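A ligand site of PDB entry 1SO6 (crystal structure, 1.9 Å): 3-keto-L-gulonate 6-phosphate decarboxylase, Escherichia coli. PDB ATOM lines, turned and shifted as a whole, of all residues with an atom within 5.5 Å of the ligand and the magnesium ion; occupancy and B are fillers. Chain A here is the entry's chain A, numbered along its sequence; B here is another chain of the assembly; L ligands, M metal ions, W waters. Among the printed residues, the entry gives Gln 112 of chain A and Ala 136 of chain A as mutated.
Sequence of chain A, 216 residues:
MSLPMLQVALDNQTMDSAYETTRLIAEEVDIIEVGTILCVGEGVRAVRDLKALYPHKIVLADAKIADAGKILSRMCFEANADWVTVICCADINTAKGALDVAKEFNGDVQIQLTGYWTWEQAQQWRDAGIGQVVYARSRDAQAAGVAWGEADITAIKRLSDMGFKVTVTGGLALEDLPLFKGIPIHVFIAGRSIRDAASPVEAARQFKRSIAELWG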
ATOM      1  N   ALA A   9     -28.575   1.677  -0.245  1.00  0.00           N
ATOM      2  CA  ALA A   9     -29.317   2.020   0.972  1.00  0.00           C
ATOM      3  C   ALA A   9     -30.683   1.358   0.877  1.00  0.00           C
ATOM      4  O   ALA A   9     -31.434   1.616  -0.072  1.00  0.00           O
ATOM      5  CB  ALA A   9     -29.493   3.548   1.156  1.00  0.00           C
ATOM      6  N   ASP A  11     -33.734   1.908   2.347  1.00  0.00           N
ATOM      7  CA  ASP A  11     -34.685   2.775   3.017  1.00  0.00           C
ATOM      8  C   ASP A  11     -36.123   2.277   2.759  1.00  0.00           C
ATOM      9  O   ASP A  11     -36.938   2.911   2.061  1.00  0.00           O
ATOM     10  CB  ASP A  11     -34.484   4.222   2.534  1.00  0.00           C
ATOM     11  CG  ASP A  11     -33.196   4.819   3.094  1.00  0.00           C
ATOM     12  OD1 ASP A  11     -33.022   4.666   4.330  1.00  0.00           O
ATOM     13  OD2 ASP A  11     -32.298   5.405   2.386  1.00  0.00           O
ATOM     14  N   GLU A  33     -26.729  -1.386   3.228  1.00  0.00           N
ATOM     15  CA  GLU A  33     -27.157  -0.517   4.297  1.00  0.00           C
ATOM     16  C   GLU A  33     -28.594  -0.848   4.746  1.00  0.00           C
ATOM     17  O   GLU A  33     -29.550  -0.872   3.932  1.00  0.00           O
ATOM     18  CB  GLU A  33     -27.085   0.967   3.871  1.00  0.00           C
ATOM     19  CG  GLU A  33     -28.046   1.881   4.664  1.00  0.00           C
ATOM     20  CD  GLU A  33     -28.014   3.324   4.259  1.00  0.00           C
ATOM     21  OE1 GLU A  33     -27.076   3.713   3.536  1.00  0.00           O
ATOM     22  OE2 GLU A  33     -28.918   4.087   4.649  1.00  0.00           O
ATOM     23  N   GLY A  35     -31.087   1.049   6.033  1.00  0.00           N
ATOM     24  CA  GLY A  35     -31.504   2.419   6.155  1.00  0.00           C
ATOM     25  C   GLY A  35     -32.200   2.789   7.449  1.00  0.00           C
ATOM     26  O   GLY A  35     -32.809   1.982   8.132  1.00  0.00           O
ATOM     27  N   THR A  36     -32.091   4.053   7.802  1.00  0.00           N
ATOM     28  CA  THR A  36     -32.718   4.537   9.019  1.00  0.00           C
ATOM     29  C   THR A  36     -34.207   4.242   8.991  1.00  0.00           C
ATOM     30  O   THR A  36     -34.797   3.915   9.991  1.00  0.00           O
ATOM     31  CB  THR A  36     -32.454   6.028   9.182  1.00  0.00           C
ATOM     32  OG1 THR A  36     -31.057   6.284   8.997  1.00  0.00           O
ATOM     33  CG2 THR A  36     -32.763   6.504  10.600  1.00  0.00           C
ATOM     34  N   ASP A  62     -27.612   2.169   9.585  1.00  0.00           N
ATOM     35  CA  ASP A  62     -27.730   3.611   9.518  1.00  0.00           C
ATOM     36  C   ASP A  62     -28.733   4.063  10.576  1.00  0.00           C
ATOM     37  O   ASP A  62     -29.823   4.573  10.321  1.00  0.00           O
ATOM     38  CB  ASP A  62     -28.119   4.037   8.119  1.00  0.00           C
ATOM     39  CG  ASP A  62     -27.970   5.546   7.882  1.00  0.00           C
ATOM     40  OD1 ASP A  62     -27.490   6.296   8.764  1.00  0.00           O
ATOM     41  OD2 ASP A  62     -28.361   6.035   6.819  1.00  0.00           O
ATOM     42  N   LYS A  64     -28.093   6.496  12.828  1.00  0.00           N
ATOM     43  CA  LYS A  64     -27.959   7.934  13.074  1.00  0.00           C
ATOM     44  C   LYS A  64     -28.047   8.209  14.578  1.00  0.00           C
ATOM     45  O   LYS A  64     -28.829   9.014  15.047  1.00  0.00           O
ATOM     46  CB  LYS A  64     -29.029   8.735  12.280  1.00  0.00           C
ATOM     47  CG  LYS A  64     -28.899   8.659  10.750  1.00  0.00           C
ATOM     48  CD  LYS A  64     -29.976   9.525  10.035  1.00  0.00           C
ATOM     49  CE  LYS A  64     -29.644   9.798   8.547  1.00  0.00           C
ATOM     50  NZ  LYS A  64     -29.541   8.554   7.695  1.00  0.00           N
ATOM     51  N   GLN A 112     -22.477  10.817  10.483  1.00  0.00           N
ATOM     52  CA  GLN A 112     -23.377  11.201   9.388  1.00  0.00           C
ATOM     53  C   GLN A 112     -23.543  12.714   9.421  1.00  0.00           C
ATOM     54  O   GLN A 112     -24.085  13.279  10.357  1.00  0.00           O
ATOM     55  CB  GLN A 112     -24.718  10.512   9.511  1.00  0.00           C
ATOM     56  CG  GLN A 112     -25.648  10.807   8.332  1.00  0.00           C
ATOM     57  CD  GLN A 112     -25.703   9.689   7.345  1.00  0.00           C
ATOM     58  OE1 GLN A 112     -24.944   8.706   7.453  1.00  0.00           O
ATOM     59  NE2 GLN A 112     -26.598   9.819   6.371  1.00  0.00           N
ATOM     60  N   THR A 114     -25.386  15.281   8.165  1.00  0.00           N
ATOM     61  CA  THR A 114     -26.638  15.718   7.561  1.00  0.00           C
ATOM     62  C   THR A 114     -27.127  16.876   8.413  1.00  0.00           C
ATOM     63  O   THR A 114     -27.163  16.776   9.646  1.00  0.00           O
ATOM     64  CB  THR A 114     -27.693  14.573   7.522  1.00  0.00           C
ATOM     65  OG1 THR A 114     -27.168  13.402   6.850  1.00  0.00           O
ATOM     66  CG2 THR A 114     -28.840  14.940   6.671  1.00  0.00           C
ATOM     67  N   ALA A 136     -23.564  13.771   3.544  1.00  0.00           N
ATOM     68  CA  ALA A 136     -24.914  13.404   3.131  1.00  0.00           C
ATOM     69  C   ALA A 136     -25.708  14.626   2.762  1.00  0.00           C
ATOM     70  O   ALA A 136     -26.048  15.485   3.607  1.00  0.00           O
ATOM     71  CB  ALA A 136     -25.599  12.638   4.255  1.00  0.00           C
ATOM     72  N   ARG A 137     -26.240  14.936   1.442  1.00  0.00           N
ATOM     73  CA  ARG A 137     -27.255  15.926   1.242  1.00  0.00           C
ATOM     74  C   ARG A 137     -28.544  15.362   1.807  1.00  0.00           C
ATOM     75  O   ARG A 137     -28.959  14.246   1.453  1.00  0.00           O
ATOM     76  CB  ARG A 137     -27.405  16.178  -0.243  1.00  0.00           C
ATOM     77  CG  ARG A 137     -28.517  17.112  -0.613  1.00  0.00           C
ATOM     78  CD  ARG A 137     -28.590  17.404  -2.049  1.00  0.00           C
ATOM     79  NE  ARG A 137     -28.758  16.200  -2.874  1.00  0.00           N
ATOM     80  CZ  ARG A 137     -29.041  16.223  -4.161  1.00  0.00           C
ATOM     81  NH1 ARG A 137     -29.193  17.364  -4.797  1.00  0.00           N
ATOM     82  NH2 ARG A 137     -29.149  15.094  -4.847  1.00  0.00           N
ATOM     83  N   SER A 138     -29.260  16.088   2.697  1.00  0.00           N
ATOM     84  CA  SER A 138     -30.534  15.617   3.267  1.00  0.00           C
ATOM     85  C   SER A 138     -31.532  15.387   2.131  1.00  0.00           C
ATOM     86  O   SER A 138     -31.652  16.194   1.208  1.00  0.00           O
ATOM     87  CB  SER A 138     -31.056  16.651   4.248  1.00  0.00           C
ATOM     88  OG  SER A 138     -32.455  16.758   4.241  1.00  0.00           O
ATOM     89  N   ARG A 139     -32.270  14.299   2.219  1.00  0.00           N
ATOM     90  CA  ARG A 139     -33.417  14.057   1.347  1.00  0.00           C
ATOM     91  C   ARG A 139     -34.402  15.254   1.252  1.00  0.00           C
ATOM     92  O   ARG A 139     -34.929  15.580   0.200  1.00  0.00           O
ATOM     93  CB  ARG A 139     -34.163  12.838   1.876  1.00  0.00           C
ATOM     94  CG  ARG A 139     -35.480  12.568   1.202  1.00  0.00           C
ATOM     95  CD  ARG A 139     -36.244  11.449   1.829  1.00  0.00           C
ATOM     96  NE  ARG A 139     -35.483  10.197   1.887  1.00  0.00           N
ATOM     97  CZ  ARG A 139     -35.649   9.143   1.067  1.00  0.00           C
ATOM     98  NH1 ARG A 139     -36.541   9.161   0.056  1.00  0.00           N
ATOM     99  NH2 ARG A 139     -34.890   8.074   1.239  1.00  0.00           N
ATOM    100  N   GLN A 142     -32.676  18.269  -0.537  1.00  0.00           N
ATOM    101  CA  GLN A 142     -32.800  17.888  -1.955  1.00  0.00           C
ATOM    102  C   GLN A 142     -34.229  18.155  -2.472  1.00  0.00           C
ATOM    103  O   GLN A 142     -34.403  18.727  -3.541  1.00  0.00           O
ATOM    104  CB  GLN A 142     -32.426  16.413  -2.125  1.00  0.00           C
ATOM    105  CG  GLN A 142     -32.642  15.872  -3.532  1.00  0.00           C
ATOM    106  CD  GLN A 142     -32.572  14.380  -3.621  1.00  0.00           C
ATOM    107  OE1 GLN A 142     -32.243  13.712  -2.644  1.00  0.00           O
ATOM    108  NE2 GLN A 142     -32.900  13.837  -4.817  1.00  0.00           N
ATOM    109  N   THR A 169     -23.175  10.821  -0.344  1.00  0.00           N
ATOM    110  CA  THR A 169     -24.529  10.324  -0.585  1.00  0.00           C
ATOM    111  C   THR A 169     -25.574  11.421  -0.555  1.00  0.00           C
ATOM    112  O   THR A 169     -25.350  12.510  -0.012  1.00  0.00           O
ATOM    113  CB  THR A 169     -24.864   9.301   0.473  1.00  0.00           C
ATOM    114  OG1 THR A 169     -26.146   8.732   0.172  1.00  0.00           O
ATOM    115  CG2 THR A 169     -24.984  10.011   1.863  1.00  0.00           C
ATOM    116  N   GLY A 170     -26.723  11.125  -1.111  1.00  0.00           N
ATOM    117  CA  GLY A 170     -27.896  11.951  -0.898  1.00  0.00           C
ATOM    118  C   GLY A 170     -28.571  12.229  -2.203  1.00  0.00           C
ATOM    119  O   GLY A 170     -28.252  13.196  -2.864  1.00  0.00           O
ATOM    120  N   GLY A 171     -29.438  11.313  -2.619  1.00  0.00           N
ATOM    121  CA  GLY A 171     -30.091  11.413  -3.907  1.00  0.00           C
ATOM    122  C   GLY A 171     -29.103  11.371  -5.064  1.00  0.00           C
ATOM    123  O   GLY A 171     -29.364  11.973  -6.095  1.00  0.00           O
ATOM    124  N   LEU A 172     -27.981  10.647  -4.925  1.00  0.00           N
ATOM    125  CA  LEU A 172     -27.027  10.548  -6.028  1.00  0.00           C
ATOM    126  C   LEU A 172     -27.625   9.873  -7.236  1.00  0.00           C
ATOM    127  O   LEU A 172     -28.276   8.816  -7.100  1.00  0.00           O
ATOM    128  CB  LEU A 172     -25.766   9.778  -5.666  1.00  0.00           C
ATOM    129  CG  LEU A 172     -24.807  10.557  -4.780  1.00  0.00           C
ATOM    130  CD1 LEU A 172     -23.677   9.653  -4.347  1.00  0.00           C
ATOM    131  CD2 LEU A 172     -24.242  11.784  -5.456  1.00  0.00           C
ATOM    132  N   ILE A 189     -22.978   5.968  -1.893  1.00  0.00           N
ATOM    133  CA  ILE A 189     -24.291   5.371  -1.632  1.00  0.00           C
ATOM    134  C   ILE A 189     -25.357   5.767  -2.675  1.00  0.00           C
ATOM    135  O   ILE A 189     -25.493   6.945  -3.043  1.00  0.00           O
ATOM    136  CB  ILE A 189     -24.814   5.822  -0.260  1.00  0.00           C
ATOM    137  CG1 ILE A 189     -23.789   5.634   0.873  1.00  0.00           C
ATOM    138  CG2 ILE A 189     -26.041   5.034   0.082  1.00  0.00           C
ATOM    139  CD1 ILE A 189     -24.347   6.103   2.214  1.00  0.00           C
ATOM    140  N   ALA A 190     -26.149   4.776  -3.092  1.00  0.00           N
ATOM    141  CA  ALA A 190     -27.372   5.011  -3.852  1.00  0.00           C
ATOM    142  C   ALA A 190     -28.486   4.216  -3.234  1.00  0.00           C
ATOM    143  O   ALA A 190     -28.337   2.985  -2.995  1.00  0.00           O
ATOM    144  CB  ALA A 190     -27.209   4.562  -5.266  1.00  0.00           C
ATOM    145  N   GLY A 191     -29.591   4.881  -2.917  1.00  0.00           N
ATOM    146  CA  GLY A 191     -30.788   4.218  -2.452  1.00  0.00           C
ATOM    147  C   GLY A 191     -31.779   4.272  -3.606  1.00  0.00           C
ATOM    148  O   GLY A 191     -31.891   3.336  -4.385  1.00  0.00           O
ATOM    149  N   ARG A 192     -32.414   5.423  -3.790  1.00  0.00           N
ATOM    150  CA  ARG A 192     -33.523   5.513  -4.753  1.00  0.00           C
ATOM    151  C   ARG A 192     -33.088   5.239  -6.180  1.00  0.00           C
ATOM    152  O   ARG A 192     -33.789   4.554  -6.897  1.00  0.00           O
ATOM    153  CB  ARG A 192     -34.193   6.880  -4.684  1.00  0.00           C
ATOM    154  CG  ARG A 192     -35.118   7.080  -3.506  1.00  0.00           C
ATOM    155  CD  ARG A 192     -35.424   8.544  -3.258  1.00  0.00           C
ATOM    156  NE  ARG A 192     -34.271   9.192  -2.627  1.00  0.00           N
ATOM    157  CZ  ARG A 192     -34.090  10.489  -2.502  1.00  0.00           C
ATOM    158  NH1 ARG A 192     -33.007  10.961  -1.879  1.00  0.00           N
ATOM    159  NH2 ARG A 192     -35.010  11.328  -2.921  1.00  0.00           N
ATOM    160  N   SER A 193     -31.933   5.747  -6.590  1.00  0.00           N
ATOM    161  CA  SER A 193     -31.453   5.551  -7.958  1.00  0.00           C
ATOM    162  C   SER A 193     -31.050   4.061  -8.300  1.00  0.00           C
ATOM    163  O   SER A 193     -31.009   3.680  -9.500  1.00  0.00           O
ATOM    164  CB  SER A 193     -30.413   6.633  -8.317  1.00  0.00           C
ATOM    165  OG  SER A 193     -29.198   6.305  -7.687  1.00  0.00           O
ATOM    166  N   ARG A 195     -32.779   1.285  -6.069  1.00  0.00           N
ATOM    167  CA  ARG A 195     -34.026   0.567  -5.743  1.00  0.00           C
ATOM    168  C   ARG A 195     -35.149   0.861  -6.715  1.00  0.00           C
ATOM    169  O   ARG A 195     -35.975   0.005  -7.028  1.00  0.00           O
ATOM    170  CB  ARG A 195     -34.508   0.946  -4.346  1.00  0.00           C
ATOM    171  CG  ARG A 195     -33.516   0.645  -3.178  1.00  0.00           C
ATOM    172  CD  ARG A 195     -34.276   0.584  -1.853  1.00  0.00           C
ATOM    173  NE  ARG A 195     -35.181   1.739  -1.738  1.00  0.00           N
ATOM    174  CZ  ARG A 195     -34.813   2.929  -1.302  1.00  0.00           C
ATOM    175  NH1 ARG A 195     -33.575   3.119  -0.896  1.00  0.00           N
ATOM    176  NH2 ARG A 195     -35.681   3.909  -1.252  1.00  0.00           N
ATOM    177  N   ASP B  67     -33.465  13.049   9.210  1.00  0.00           N
ATOM    178  CA  ASP B  67     -33.651  13.238   7.795  1.00  0.00           C
ATOM    179  C   ASP B  67     -34.898  12.464   7.427  1.00  0.00           C
ATOM    180  O   ASP B  67     -35.395  11.696   8.217  1.00  0.00           O
ATOM    181  CB  ASP B  67     -32.433  12.710   7.017  1.00  0.00           C
ATOM    182  CG  ASP B  67     -32.403  13.211   5.571  1.00  0.00           C
ATOM    183  OD1 ASP B  67     -33.109  14.161   5.218  1.00  0.00           O
ATOM    184  OD2 ASP B  67     -31.665  12.690   4.713  1.00  0.00           O
HETATM  185  O1  LIG L   1     -30.857   9.457  -1.066  1.00  0.00           O
HETATM  186  P1  LIG L   1     -30.867   8.011  -1.495  1.00  0.00           P
HETATM  187  O2  LIG L   1     -32.273   7.510  -1.810  1.00  0.00           O
HETATM  188  O3  LIG L   1     -29.792   7.768  -2.561  1.00  0.00           O
HETATM  189  O4  LIG L   1     -30.487   7.201  -0.185  1.00  0.00           O
HETATM  190  C1  LIG L   1     -29.180   7.274   0.382  1.00  0.00           C
HETATM  191  C2  LIG L   1     -29.118   8.197   1.606  1.00  0.00           C
HETATM  192  O5  LIG L   1     -27.831   8.058   2.218  1.00  0.00           O
HETATM  193  C3  LIG L   1     -30.164   7.799   2.648  1.00  0.00           C
HETATM  194  O6  LIG L   1     -29.994   6.432   3.061  1.00  0.00           O
HETATM  195  C4  LIG L   1     -29.993   8.630   3.871  1.00  0.00           C
HETATM  196  O7  LIG L   1     -29.391   8.102   4.911  1.00  0.00           O
HETATM  197  N1  LIG L   1     -30.416   9.822   3.844  1.00  0.00           N
HETATM  198  O8  LIG L   1     -30.278  10.629   4.992  1.00  0.00           O
HETATM  199 MG    MG M   1     -29.120   6.057   4.997  1.00  0.00          MG
HETATM  200  O   HOH W   1     -27.270   6.339   4.006  1.00  0.00           O
HETATM  201  O   HOH W   2     -31.260  10.830   1.215  1.00  0.00           O
HETATM  202  O   HOH W   3     -30.221   7.870  -5.146  1.00  0.00           O
HETATM  203  O   HOH W   4     -27.440   8.859  -2.743  1.00  0.00           O
HETATM  204  O   HOH W   5     -33.334   5.827  -0.092  1.00  0.00           O
HETATM  205  O   HOH W   6     -33.364   9.362   3.698  1.00  0.00           O
HETATM  206  O   HOH W   7     -32.558   8.430   6.285  1.00  0.00           O
HETATM  207  O   HOH W   8     -31.093   5.813   5.694  1.00  0.00           O
HETATM  208  O   HOH W   9     -28.926  11.958   2.443  1.00  0.00           O
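The side-chain carboxylate of Asp 67 of chain B is in hydrogen-bond range of an oxygen (O8) of the ligand, 2.5 Å away.
OD2 of Asp 11 lies close to O6 of the ligand, 2.6 Å away.
The side-chain hydroxyl (OG1) of Thr 169 lies within hydrogen-bond range of an oxygen (O5) of the ligand, 2.7 Å away.
N of Arg 192 lies within hydrogen-bond range of O2 of the ligand.
The guanidinium group (NE) of Arg 192 is in salt-bridge range of an oxygen (O2) of the ligand, 2.7 Å away.
An oxygen (O1) of the ligand is in hydrogen-bond range of the backbone NH of Gly 171, 2.8 Å away.
NZ of Lys 64 sits at hydrogen-bond distance from O8 of the ligand, 3.5 Å away.
The backbone NH of Gly 191 is in hydrogen-bond range of an oxygen (O3) of the ligand (2.9 Å).
The side-chain carboxylate (OD1) of Asp 62 lies within salt-bridge range of the side-chain amino group (NZ) of Lys 64 (3.2 Å).
The side-chain carboxylate (OD2) of Asp 11 is in salt-bridge range of the guanidinium group (NH2) of Arg 139, at 3.9 Å.
The backbone carbonyl oxygen of Thr 169 lies within hydrogen-bond range of the backbone NH of Arg 137 (3.0 Å).
The guanidinium group of Arg 137 is in hydrogen-bond range of the backbone carbonyl oxygen of Gly 171 (3.4 Å).
NZ of Lys 64 lies close to NE2 of Gln 112, 3.5 Å away.
NZ of Lys 64 is in hydrogen-bond range of OG1 of Thr 36, 3.0 Å away.
N of Ala 9 sits at hydrogen-bond distance from O of Ala 190 (3.1 Å).
The backbone carbonyl oxygen (O) of Gly 170 sits at hydrogen-bond distance from the guanidinium group (NH2) of Arg 137 (2.9 Å).
Ala 9 touches the ligand (CB to O6, 3.5 Å).
Gln 112 touches the ligand (NE2 to O7, 3.6 Å).
C of Gly 170 touches O1 of the ligand (3.8 Å).
Ile 189 touches the ligand (CG2 to C1, 3.9 Å).
Ala 190 touches the ligand.
Hydrophobic or aromatic side chains within 4 Å of the ligand: Ala 9 and Ile 189.
Of the 25 residues printed, 14 come within 4 Å of the ligand.
The nearest printed residue that does not touch the ligand is Arg 139 (4.1 Å).
Merely in contact with the magnesium ion: Lys 64 (3.7 Å).
Within 4 Å of the magnesium ion: Glu 33, Asp 62 and Lys 64.
The nearest printed residue that does not touch the magnesium ion is Asp 11 (4.2 Å).
The magnesium ion is bound by the side-chain carboxylate of Asp 62 (2.0 Å), the side-chain carboxylate of Glu 33 (2.0 Å), an oxygen (O7) of the ligand (2.1 Å), water W8 (2.1 Å), water W1 (2.1 Å) and an oxygen (O6) of the ligand (2.2 Å).
The magnesium ion has six donor atoms within binding distance.
Water W8 bridges OD1 of Asp 11 (2.6 Å) and N of Thr 36 (2.9 Å).
Water W1 lies within hydrogen-bond range of an oxygen (O5) of the ligand (2.5 Å) and the side-chain carboxylate of Glu 33 (2.7 Å).
Water W3 lies within hydrogen-bond range of an oxygen (O3) of the ligand (2.6 Å), the backbone carbonyl oxygen of Leu 172 (2.9 Å) and the backbone NH of Ser 193 (3.1 Å).
Water W5 lies within hydrogen-bond range of an oxygen (O2) of the ligand (2.6 Å), the side-chain carboxylate of Asp 11 (2.7 Å), the guanidinium group of Arg 195 (2.8 Å) and the guanidinium group of Arg 139 (3.0 Å).
Water W9 lies within hydrogen-bond range of the backbone carbonyl oxygen (O) of Arg 137 and a nitrogen (N1) of the ligand.
Water W6 lies within hydrogen-bond range of the guanidinium group (NE) of Arg 139 (2.9 Å) and a nitrogen (N1) of the ligand (3.0 Å).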
